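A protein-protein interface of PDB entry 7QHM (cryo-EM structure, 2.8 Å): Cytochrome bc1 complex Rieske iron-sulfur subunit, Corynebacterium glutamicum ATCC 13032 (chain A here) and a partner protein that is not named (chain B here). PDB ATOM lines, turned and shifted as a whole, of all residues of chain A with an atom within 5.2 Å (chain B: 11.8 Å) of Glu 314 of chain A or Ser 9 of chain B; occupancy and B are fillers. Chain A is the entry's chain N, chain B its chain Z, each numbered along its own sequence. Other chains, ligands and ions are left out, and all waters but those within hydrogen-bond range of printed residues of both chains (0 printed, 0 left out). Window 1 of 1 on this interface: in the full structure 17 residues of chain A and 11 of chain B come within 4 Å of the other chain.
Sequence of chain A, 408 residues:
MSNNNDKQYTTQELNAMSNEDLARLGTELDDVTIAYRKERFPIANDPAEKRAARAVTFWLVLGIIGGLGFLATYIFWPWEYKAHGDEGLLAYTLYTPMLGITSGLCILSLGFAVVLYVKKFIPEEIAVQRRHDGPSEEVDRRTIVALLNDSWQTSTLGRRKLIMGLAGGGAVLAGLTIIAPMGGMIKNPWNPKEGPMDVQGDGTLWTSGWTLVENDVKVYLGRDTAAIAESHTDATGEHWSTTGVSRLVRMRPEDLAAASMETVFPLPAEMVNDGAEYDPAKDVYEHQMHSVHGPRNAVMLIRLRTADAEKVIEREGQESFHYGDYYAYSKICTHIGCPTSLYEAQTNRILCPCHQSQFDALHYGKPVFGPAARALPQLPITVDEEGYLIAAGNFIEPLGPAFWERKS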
ATOM      1  N   VAL A 312      23.641 -24.156 -15.840  1.00  0.00           N
ATOM      2  CA  VAL A 312      23.722 -23.222 -16.951  1.00  0.00           C
ATOM      3  C   VAL A 312      25.172 -22.849 -17.218  1.00  0.00           C
ATOM      4  O   VAL A 312      25.961 -22.629 -16.290  1.00  0.00           O
ATOM      5  CB  VAL A 312      22.869 -21.979 -16.639  1.00  0.00           C
ATOM      6  CG1 VAL A 312      23.146 -20.856 -17.609  1.00  0.00           C
ATOM      7  CG2 VAL A 312      21.404 -22.338 -16.658  1.00  0.00           C
ATOM      8  N   ILE A 313      25.525 -22.766 -18.497  1.00  0.00           N
ATOM      9  CA  ILE A 313      26.793 -22.211 -18.951  1.00  0.00           C
ATOM     10  C   ILE A 313      26.489 -20.863 -19.586  1.00  0.00           C
ATOM     11  O   ILE A 313      25.799 -20.797 -20.607  1.00  0.00           O
ATOM     12  CB  ILE A 313      27.504 -23.156 -19.930  1.00  0.00           C
ATOM     13  CG1 ILE A 313      28.079 -24.343 -19.163  1.00  0.00           C
ATOM     14  CG2 ILE A 313      28.613 -22.435 -20.674  1.00  0.00           C
ATOM     15  CD1 ILE A 313      28.426 -25.539 -20.008  1.00  0.00           C
ATOM     16  N   GLU A 314      26.991 -19.793 -18.982  1.00  0.00           N
ATOM     17  CA  GLU A 314      26.722 -18.452 -19.472  1.00  0.00           C
ATOM     18  C   GLU A 314      27.597 -18.140 -20.684  1.00  0.00           C
ATOM     19  O   GLU A 314      28.569 -18.839 -20.981  1.00  0.00           O
ATOM     20  CB  GLU A 314      26.976 -17.415 -18.377  1.00  0.00           C
ATOM     21  CG  GLU A 314      26.208 -17.626 -17.079  1.00  0.00           C
ATOM     22  CD  GLU A 314      24.725 -17.353 -17.203  1.00  0.00           C
ATOM     23  OE1 GLU A 314      24.332 -16.443 -17.962  1.00  0.00           O
ATOM     24  OE2 GLU A 314      23.945 -18.052 -16.531  1.00  0.00           O
ATOM     25  N   ARG A 315      27.248 -17.068 -21.386  1.00  0.00           N
ATOM     26  CA  ARG A 315      28.101 -16.530 -22.429  1.00  0.00           C
ATOM     27  C   ARG A 315      29.026 -15.475 -21.839  1.00  0.00           C
ATOM     28  O   ARG A 315      28.704 -14.835 -20.836  1.00  0.00           O
ATOM     29  CB  ARG A 315      27.275 -15.920 -23.564  1.00  0.00           C
ATOM     30  CG  ARG A 315      28.022 -15.894 -24.889  1.00  0.00           C
ATOM     31  CD  ARG A 315      27.572 -14.819 -25.837  1.00  0.00           C
ATOM     32  NE  ARG A 315      26.297 -15.115 -26.470  1.00  0.00           N
ATOM     33  CZ  ARG A 315      25.850 -14.543 -27.579  1.00  0.00           C
ATOM     34  NH1 ARG A 315      26.576 -13.678 -28.258  1.00  0.00           N
ATOM     35  NH2 ARG A 315      24.638 -14.849 -28.019  1.00  0.00           N
ATOM     36  N   GLU A 316      30.192 -15.321 -22.458  1.00  0.00           N
ATOM     37  CA  GLU A 316      31.119 -14.252 -22.115  1.00  0.00           C
ATOM     38  C   GLU A 316      30.425 -12.894 -22.164  1.00  0.00           C
ATOM     39  O   GLU A 316      29.760 -12.555 -23.143  1.00  0.00           O
ATOM     40  CB  GLU A 316      32.306 -14.301 -23.083  1.00  0.00           C
ATOM     41  CG  GLU A 316      33.219 -13.073 -23.151  1.00  0.00           C
ATOM     42  CD  GLU A 316      33.911 -12.747 -21.840  1.00  0.00           C
ATOM     43  OE1 GLU A 316      33.734 -13.491 -20.855  1.00  0.00           O
ATOM     44  OE2 GLU A 316      34.643 -11.738 -21.797  1.00  0.00           O
ATOM     45  N   GLN A 318      27.888 -11.859 -20.420  1.00  0.00           N
ATOM     46  CA  GLN A 318      26.458 -11.922 -20.154  1.00  0.00           C
ATOM     47  C   GLN A 318      26.178 -12.794 -18.953  1.00  0.00           C
ATOM     48  O   GLN A 318      25.188 -13.522 -18.911  1.00  0.00           O
ATOM     49  CB  GLN A 318      25.703 -12.450 -21.368  1.00  0.00           C
ATOM     50  CG  GLN A 318      25.851 -11.601 -22.597  1.00  0.00           C
ATOM     51  CD  GLN A 318      25.403 -12.311 -23.840  1.00  0.00           C
ATOM     52  OE1 GLN A 318      24.649 -13.278 -23.782  1.00  0.00           O
ATOM     53  NE2 GLN A 318      25.870 -11.836 -24.982  1.00  0.00           N
ATOM     54  N   GLU A 319      27.040 -12.731 -17.945  1.00  0.00           N
ATOM     55  CA  GLU A 319      26.888 -13.616 -16.801  1.00  0.00           C
ATOM     56  C   GLU A 319      25.876 -13.097 -15.797  1.00  0.00           C
ATOM     57  O   GLU A 319      25.312 -13.895 -15.041  1.00  0.00           O
ATOM     58  CB  GLU A 319      28.234 -13.831 -16.109  1.00  0.00           C
ATOM     59  CG  GLU A 319      29.332 -14.355 -17.021  1.00  0.00           C
ATOM     60  CD  GLU A 319      30.058 -13.259 -17.763  1.00  0.00           C
ATOM     61  OE1 GLU A 319      29.515 -12.141 -17.832  1.00  0.00           O
ATOM     62  OE2 GLU A 319      31.165 -13.512 -18.276  1.00  0.00           O
ATOM     63  N   HIS A 322      20.708 -12.729 -16.055  1.00  0.00           N
ATOM     64  CA  HIS A 322      19.567 -13.396 -15.459  1.00  0.00           C
ATOM     65  C   HIS A 322      19.197 -12.748 -14.131  1.00  0.00           C
ATOM     66  O   HIS A 322      19.818 -11.784 -13.680  1.00  0.00           O
ATOM     67  CB  HIS A 322      19.859 -14.879 -15.278  1.00  0.00           C
ATOM     68  CG  HIS A 322      21.044 -15.166 -14.413  1.00  0.00           C
ATOM     69  ND1 HIS A 322      20.950 -15.343 -13.051  1.00  0.00           N
ATOM     70  CD2 HIS A 322      22.352 -15.315 -14.723  1.00  0.00           C
ATOM     71  CE1 HIS A 322      22.149 -15.588 -12.558  1.00  0.00           C
ATOM     72  NE2 HIS A 322      23.019 -15.575 -13.553  1.00  0.00           N
ATOM     73  N   TYR A 327      15.433 -16.261 -16.914  1.00  0.00           N
ATOM     74  CA  TYR A 327      16.234 -15.952 -18.086  1.00  0.00           C
ATOM     75  C   TYR A 327      15.317 -15.407 -19.166  1.00  0.00           C
ATOM     76  O   TYR A 327      14.149 -15.771 -19.238  1.00  0.00           O
ATOM     77  CB  TYR A 327      16.961 -17.186 -18.600  1.00  0.00           C
ATOM     78  CG  TYR A 327      18.117 -17.617 -17.743  1.00  0.00           C
ATOM     79  CD1 TYR A 327      17.913 -18.289 -16.556  1.00  0.00           C
ATOM     80  CD2 TYR A 327      19.410 -17.356 -18.124  1.00  0.00           C
ATOM     81  CE1 TYR A 327      18.963 -18.680 -15.777  1.00  0.00           C
ATOM     82  CE2 TYR A 327      20.462 -17.747 -17.352  1.00  0.00           C
ATOM     83  CZ  TYR A 327      20.233 -18.404 -16.179  1.00  0.00           C
ATOM     84  OH  TYR A 327      21.295 -18.797 -15.408  1.00  0.00           O
ATOM     85  N   TYR A 364      23.384 -20.775 -22.980  1.00  0.00           N
ATOM     86  CA  TYR A 364      23.232 -19.405 -23.485  1.00  0.00           C
ATOM     87  C   TYR A 364      22.583 -19.336 -24.864  1.00  0.00           C
ATOM     88  O   TYR A 364      22.825 -18.402 -25.628  1.00  0.00           O
ATOM     89  CB  TYR A 364      24.564 -18.642 -23.469  1.00  0.00           C
ATOM     90  CG  TYR A 364      25.731 -19.219 -24.230  1.00  0.00           C
ATOM     91  CD1 TYR A 364      25.841 -19.077 -25.598  1.00  0.00           C
ATOM     92  CD2 TYR A 364      26.755 -19.867 -23.565  1.00  0.00           C
ATOM     93  CE1 TYR A 364      26.924 -19.594 -26.285  1.00  0.00           C
ATOM     94  CE2 TYR A 364      27.842 -20.378 -24.240  1.00  0.00           C
ATOM     95  CZ  TYR A 364      27.921 -20.239 -25.595  1.00  0.00           C
ATOM     96  OH  TYR A 364      29.002 -20.751 -26.263  1.00  0.00           O
ATOM     97  N   GLN A 378      20.242 -12.683 -25.557  1.00  0.00           N
ATOM     98  CA  GLN A 378      19.732 -12.702 -24.195  1.00  0.00           C
ATOM     99  C   GLN A 378      19.476 -11.277 -23.726  1.00  0.00           C
ATOM    100  O   GLN A 378      20.301 -10.389 -23.943  1.00  0.00           O
ATOM    101  CB  GLN A 378      20.730 -13.388 -23.274  1.00  0.00           C
ATOM    102  CG  GLN A 378      20.245 -13.611 -21.878  1.00  0.00           C
ATOM    103  CD  GLN A 378      21.186 -14.463 -21.089  1.00  0.00           C
ATOM    104  OE1 GLN A 378      22.159 -14.987 -21.622  1.00  0.00           O
ATOM    105  NE2 GLN A 378      20.905 -14.618 -19.810  1.00  0.00           N
ATOM    106  N   PRO B   4      32.936 -15.179 -34.077  1.00  0.00           N
ATOM    107  CA  PRO B   4      34.061 -14.852 -33.195  1.00  0.00           C
ATOM    108  C   PRO B   4      33.688 -14.126 -31.909  1.00  0.00           C
ATOM    109  O   PRO B   4      34.595 -13.717 -31.180  1.00  0.00           O
ATOM    110  CB  PRO B   4      34.929 -13.953 -34.085  1.00  0.00           C
ATOM    111  CG  PRO B   4      33.963 -13.260 -34.934  1.00  0.00           C
ATOM    112  CD  PRO B   4      32.900 -14.267 -35.237  1.00  0.00           C
ATOM    113  N   HIS B   5      32.403 -13.940 -31.606  1.00  0.00           N
ATOM    114  CA  HIS B   5      31.964 -13.317 -30.362  1.00  0.00           C
ATOM    115  C   HIS B   5      30.805 -14.122 -29.775  1.00  0.00           C
ATOM    116  O   HIS B   5      29.676 -13.662 -29.658  1.00  0.00           O
ATOM    117  CB  HIS B   5      31.562 -11.863 -30.588  1.00  0.00           C
ATOM    118  CG  HIS B   5      32.710 -10.966 -30.926  1.00  0.00           C
ATOM    119  ND1 HIS B   5      33.511 -10.389 -29.965  1.00  0.00           N
ATOM    120  CD2 HIS B   5      33.191 -10.544 -32.120  1.00  0.00           C
ATOM    121  CE1 HIS B   5      34.436  -9.650 -30.552  1.00  0.00           C
ATOM    122  NE2 HIS B   5      34.265  -9.728 -31.859  1.00  0.00           N
ATOM    123  N   GLN B   6      31.100 -15.357 -29.389  1.00  0.00           N
ATOM    124  CA  GLN B   6      30.098 -16.270 -28.870  1.00  0.00           C
ATOM    125  C   GLN B   6      30.813 -17.314 -28.033  1.00  0.00           C
ATOM    126  O   GLN B   6      30.724 -18.512 -28.310  1.00  0.00           O
ATOM    127  CB  GLN B   6      29.312 -16.906 -30.016  1.00  0.00           C
ATOM    128  CG  GLN B   6      28.079 -17.677 -29.609  1.00  0.00           C
ATOM    129  CD  GLN B   6      27.261 -18.126 -30.805  1.00  0.00           C
ATOM    130  OE1 GLN B   6      26.675 -17.312 -31.508  1.00  0.00           O
ATOM    131  NE2 GLN B   6      27.230 -19.427 -31.043  1.00  0.00           N
ATOM    132  N   GLN B   7      31.543 -16.854 -27.024  1.00  0.00           N
ATOM    133  CA  GLN B   7      32.369 -17.695 -26.176  1.00  0.00           C
ATOM    134  C   GLN B   7      31.613 -18.108 -24.922  1.00  0.00           C
ATOM    135  O   GLN B   7      30.636 -17.481 -24.524  1.00  0.00           O
ATOM    136  CB  GLN B   7      33.646 -16.960 -25.769  1.00  0.00           C
ATOM    137  CG  GLN B   7      34.692 -16.853 -26.853  1.00  0.00           C
ATOM    138  CD  GLN B   7      34.344 -15.832 -27.914  1.00  0.00           C
ATOM    139  OE1 GLN B   7      33.758 -14.787 -27.624  1.00  0.00           O
ATOM    140  NE2 GLN B   7      34.705 -16.129 -29.155  1.00  0.00           N
ATOM    141  N   ASP B   8      32.082 -19.176 -24.297  1.00  0.00           N
ATOM    142  CA  ASP B   8      31.631 -19.485 -22.953  1.00  0.00           C
ATOM    143  C   ASP B   8      32.254 -18.500 -21.979  1.00  0.00           C
ATOM    144  O   ASP B   8      33.364 -18.008 -22.188  1.00  0.00           O
ATOM    145  CB  ASP B   8      32.013 -20.911 -22.559  1.00  0.00           C
ATOM    146  CG  ASP B   8      31.632 -21.922 -23.606  1.00  0.00           C
ATOM    147  OD1 ASP B   8      30.659 -21.671 -24.342  1.00  0.00           O
ATOM    148  OD2 ASP B   8      32.302 -22.969 -23.698  1.00  0.00           O
ATOM    149  N   SER B   9      31.531 -18.196 -20.920  1.00  0.00           N
ATOM    150  CA  SER B   9      32.075 -17.296 -19.920  1.00  0.00           C
ATOM    151  C   SER B   9      33.229 -18.004 -19.218  1.00  0.00           C
ATOM    152  O   SER B   9      33.073 -19.158 -18.811  1.00  0.00           O
ATOM    153  CB  SER B   9      31.004 -16.884 -18.915  1.00  0.00           C
ATOM    154  OG  SER B   9      30.504 -17.996 -18.206  1.00  0.00           O
ATOM    155  N   PRO B  10      34.406 -17.383 -19.091  1.00  0.00           N
ATOM    156  CA  PRO B  10      35.450 -18.048 -18.297  1.00  0.00           C
ATOM    157  C   PRO B  10      35.048 -18.218 -16.846  1.00  0.00           C
ATOM    158  O   PRO B  10      35.248 -19.290 -16.265  1.00  0.00           O
ATOM    159  CB  PRO B  10      36.660 -17.118 -18.460  1.00  0.00           C
ATOM    160  CG  PRO B  10      36.399 -16.366 -19.698  1.00  0.00           C
ATOM    161  CD  PRO B  10      34.927 -16.166 -19.740  1.00  0.00           C
ATOM    162  N   VAL B  11      34.463 -17.189 -16.252  1.00  0.00           N
ATOM    163  CA  VAL B  11      34.079 -17.223 -14.847  1.00  0.00           C
ATOM    164  C   VAL B  11      32.821 -18.061 -14.691  1.00  0.00           C
ATOM    165  O   VAL B  11      31.881 -17.957 -15.486  1.00  0.00           O
ATOM    166  CB  VAL B  11      33.883 -15.793 -14.303  1.00  0.00           C
ATOM    167  CG1 VAL B  11      32.748 -15.041 -15.033  1.00  0.00           C
ATOM    168  CG2 VAL B  11      33.636 -15.821 -12.798  1.00  0.00           C
ATOM    169  N   GLN B  12      32.802 -18.896 -13.662  1.00  0.00           N
ATOM    170  CA  GLN B  12      31.668 -19.766 -13.397  1.00  0.00           C
ATOM    171  C   GLN B  12      30.611 -19.026 -12.586  1.00  0.00           C
ATOM    172  O   GLN B  12      30.897 -18.049 -11.891  1.00  0.00           O
ATOM    173  CB  GLN B  12      32.117 -21.028 -12.656  1.00  0.00           C
ATOM    174  CG  GLN B  12      32.645 -20.785 -11.249  1.00  0.00           C
ATOM    175  CD  GLN B  12      33.242 -22.028 -10.631  1.00  0.00           C
ATOM    176  OE1 GLN B  12      33.489 -23.020 -11.316  1.00  0.00           O
ATOM    177  NE2 GLN B  12      33.476 -21.984  -9.325  1.00  0.00           N
ATOM    178  N   ARG B  13      29.375 -19.504 -12.689  1.00  0.00           N
ATOM    179  CA  ARG B  13      28.292 -18.933 -11.900  1.00  0.00           C
ATOM    180  C   ARG B  13      28.524 -19.233 -10.427  1.00  0.00           C
ATOM    181  O   ARG B  13      28.768 -20.382 -10.049  1.00  0.00           O
ATOM    182  CB  ARG B  13      26.944 -19.484 -12.362  1.00  0.00           C
ATOM    183  CG  ARG B  13      26.789 -20.991 -12.235  1.00  0.00           C
ATOM    184  CD  ARG B  13      25.521 -21.484 -12.927  1.00  0.00           C
ATOM    185  NE  ARG B  13      24.310 -21.083 -12.214  1.00  0.00           N
ATOM    186  CZ  ARG B  13      23.512 -20.071 -12.532  1.00  0.00           C
ATOM    187  NH1 ARG B  13      23.735 -19.303 -13.585  1.00  0.00           N
ATOM    188  NH2 ARG B  13      22.456 -19.821 -11.767  1.00  0.00           N
ATOM    189  N   THR B  14      28.451 -18.198  -9.595  1.00  0.00           N
ATOM    190  CA  THR B  14      28.890 -18.279  -8.209  1.00  0.00           C
ATOM    191  C   THR B  14      27.767 -18.616  -7.233  1.00  0.00           C
ATOM    192  O   THR B  14      28.009 -18.620  -6.022  1.00  0.00           O
ATOM    193  CB  THR B  14      29.564 -16.960  -7.793  1.00  0.00           C
ATOM    194  OG1 THR B  14      30.197 -17.120  -6.516  1.00  0.00           O
ATOM    195  CG2 THR B  14      28.561 -15.797  -7.724  1.00  0.00           C
ATOM    196  N   ASN B  15      26.558 -18.901  -7.720  1.00  0.00           N
ATOM    197  CA  ASN B  15      25.413 -19.203  -6.861  1.00  0.00           C
ATOM    198  C   ASN B  15      25.117 -18.021  -5.934  1.00  0.00           C
ATOM    199  O   ASN B  15      25.170 -18.122  -4.709  1.00  0.00           O
ATOM    200  CB  ASN B  15      25.658 -20.489  -6.064  1.00  0.00           C
ATOM    201  CG  ASN B  15      24.413 -20.989  -5.363  1.00  0.00           C
ATOM    202  OD1 ASN B  15      23.303 -20.525  -5.628  1.00  0.00           O
ATOM    203  ND2 ASN B  15      24.592 -21.950  -4.462  1.00  0.00           N
ATOM    204  N   GLU B  16      24.808 -16.886  -6.557  1.00  0.00           N
ATOM    205  CA  GLU B  16      24.612 -15.638  -5.833  1.00  0.00           C
ATOM    206  C   GLU B  16      23.264 -15.651  -5.106  1.00  0.00           C
ATOM    207  O   GLU B  16      22.541 -16.651  -5.099  1.00  0.00           O
ATOM    208  CB  GLU B  16      24.735 -14.453  -6.793  1.00  0.00           C
ATOM    209  CG  GLU B  16      23.732 -14.429  -7.943  1.00  0.00           C
ATOM    210  CD  GLU B  16      23.979 -13.276  -8.895  1.00  0.00           C
ATOM    211  OE1 GLU B  16      24.179 -12.141  -8.418  1.00  0.00           O
ATOM    212  OE2 GLU B  16      23.984 -13.509 -10.124  1.00  0.00           O
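O of Val 312 of chain A touches CD of Arg 13 of chain B, at 3.6 Å. Arg 315 of chain A touches Gln 7 of chain B. Arg 315 of chain A touches Ser 9 of chain B. C of Asp 8 of chain B touches N of Glu 316 of chain A, 3.8 Å away. N of Ser 9 of chain B touches N of Glu 316 of chain A, at 3.5 Å. CD of Pro 10 of chain B touches OE1 of Glu 316 of chain A (3.1 Å). Glu 319 of chain A touches Ser 9 of chain B (OE2 to CB, 3.4 Å). Glu 319 of chain A touches Val 11 of chain B. OE2 of Glu 16 of chain B touches CE1 of His 322 of chain A (3.7 Å). Tyr 364 of chain A touches Gln 7 of chain B.
The backbone carbonyl oxygen (O) of Ile 313 of chain A lies close to the backbone NH (N) of Tyr 364 of chain A. OH of Tyr 327 of chain A lies within hydrogen-bond range of OE2 of Glu 314 of chain A (3.0 Å). A ring nitrogen (NE2) of His 322 of chain A lies within hydrogen-bond range of the backbone carbonyl oxygen of Glu 319 of chain A, 3.2 Å away. The backbone carbonyl oxygen (O) of Pro 4 of chain B is in hydrogen-bond range of the side-chain amide nitrogen (NE2) of Gln 7 of chain B, 3.2 Å away. The backbone carbonyl oxygen (O) of Val 11 of chain B is in hydrogen-bond range of the side-chain hydroxyl (OG) of Ser 9 of chain B (3.0 Å).
The backbone carbonyl oxygen (O) of Glu 314 of chain A sits at hydrogen-bond distance from the backbone NH (N) of Ser 9 of chain B (3.0 Å). The guanidinium group (NH1) of Arg 13 of chain B is in salt-bridge range of the side-chain carboxylate (OE2) of Glu 314 of chain A (3.2 Å). NH1 of Arg 315 of chain A lies within hydrogen-bond range of O of His 5 of chain B. The backbone carbonyl oxygen of Gln 7 of chain B sits at hydrogen-bond distance from the backbone NH of Glu 316 of chain A. OH of Tyr 327 of chain A is in hydrogen-bond range of NH1 of Arg 13 of chain B, at 3.1 Å. The backbone carbonyl oxygen of Gln 6 of chain B sits at hydrogen-bond distance from the side-chain hydroxyl of Tyr 364 of chain A, at 3.5 Å. The side-chain carboxylate (OD1) of Asp 8 of chain B is in hydrogen-bond range of the side-chain hydroxyl (OH) of Tyr 364 of chain A.
Hydrophobic or aromatic side chains of chain B within 4 Å of the printed part of chain A: Pro 10 and Val 11. Along chain A the printed residues that touch a printed residue of chain B span positions 312 to 364. Among the printed residues, 19 pairs touch across the chains. Among the printed residues, Asp or Glu carboxylates within 4 Å of a Lys or Arg side-chain nitrogen of the other chain: Glu 314 of chain A with Arg 13 of chain B (3.2 Å).
Glu 314 of chain A touches three residues of chain B. Of chain A, only Glu 314, Arg 315, Glu 316 and Glu 319 come within 4 Å of Ser 9 of chain B. Val 312 of chain A touches just one residue of chain B: Arg 13. No residue of chain B comes within 4 Å of Ile 313 of chain A. Printed residues of chain B within 4 Å of Glu 316 of chain A: Gln 7, Asp 8, Ser 9 and Pro 10. Glu 319 of chain A touches two residues of chain B. Of the printed residues of chain A, Asp 8 of chain B touches Glu 314, Glu 316 and Tyr 364. Printed residues of chain B within 4 Å of Arg 315 of chain A: His 5 (3.4 Å), Gln 7 (3.1 Å) and Ser 9 (3.6 Å). Of the printed residues of chain B, Tyr 327 of chain A touches Arg 13 (3.1 Å). The nearest residue of chain A that does not touch Ser 9 of chain B is Ile 313 of chain A (5.1 Å). The nearest printed residue of chain A that does not touch Gln 7 of chain B is Glu 314 of chain A (4.3 Å).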
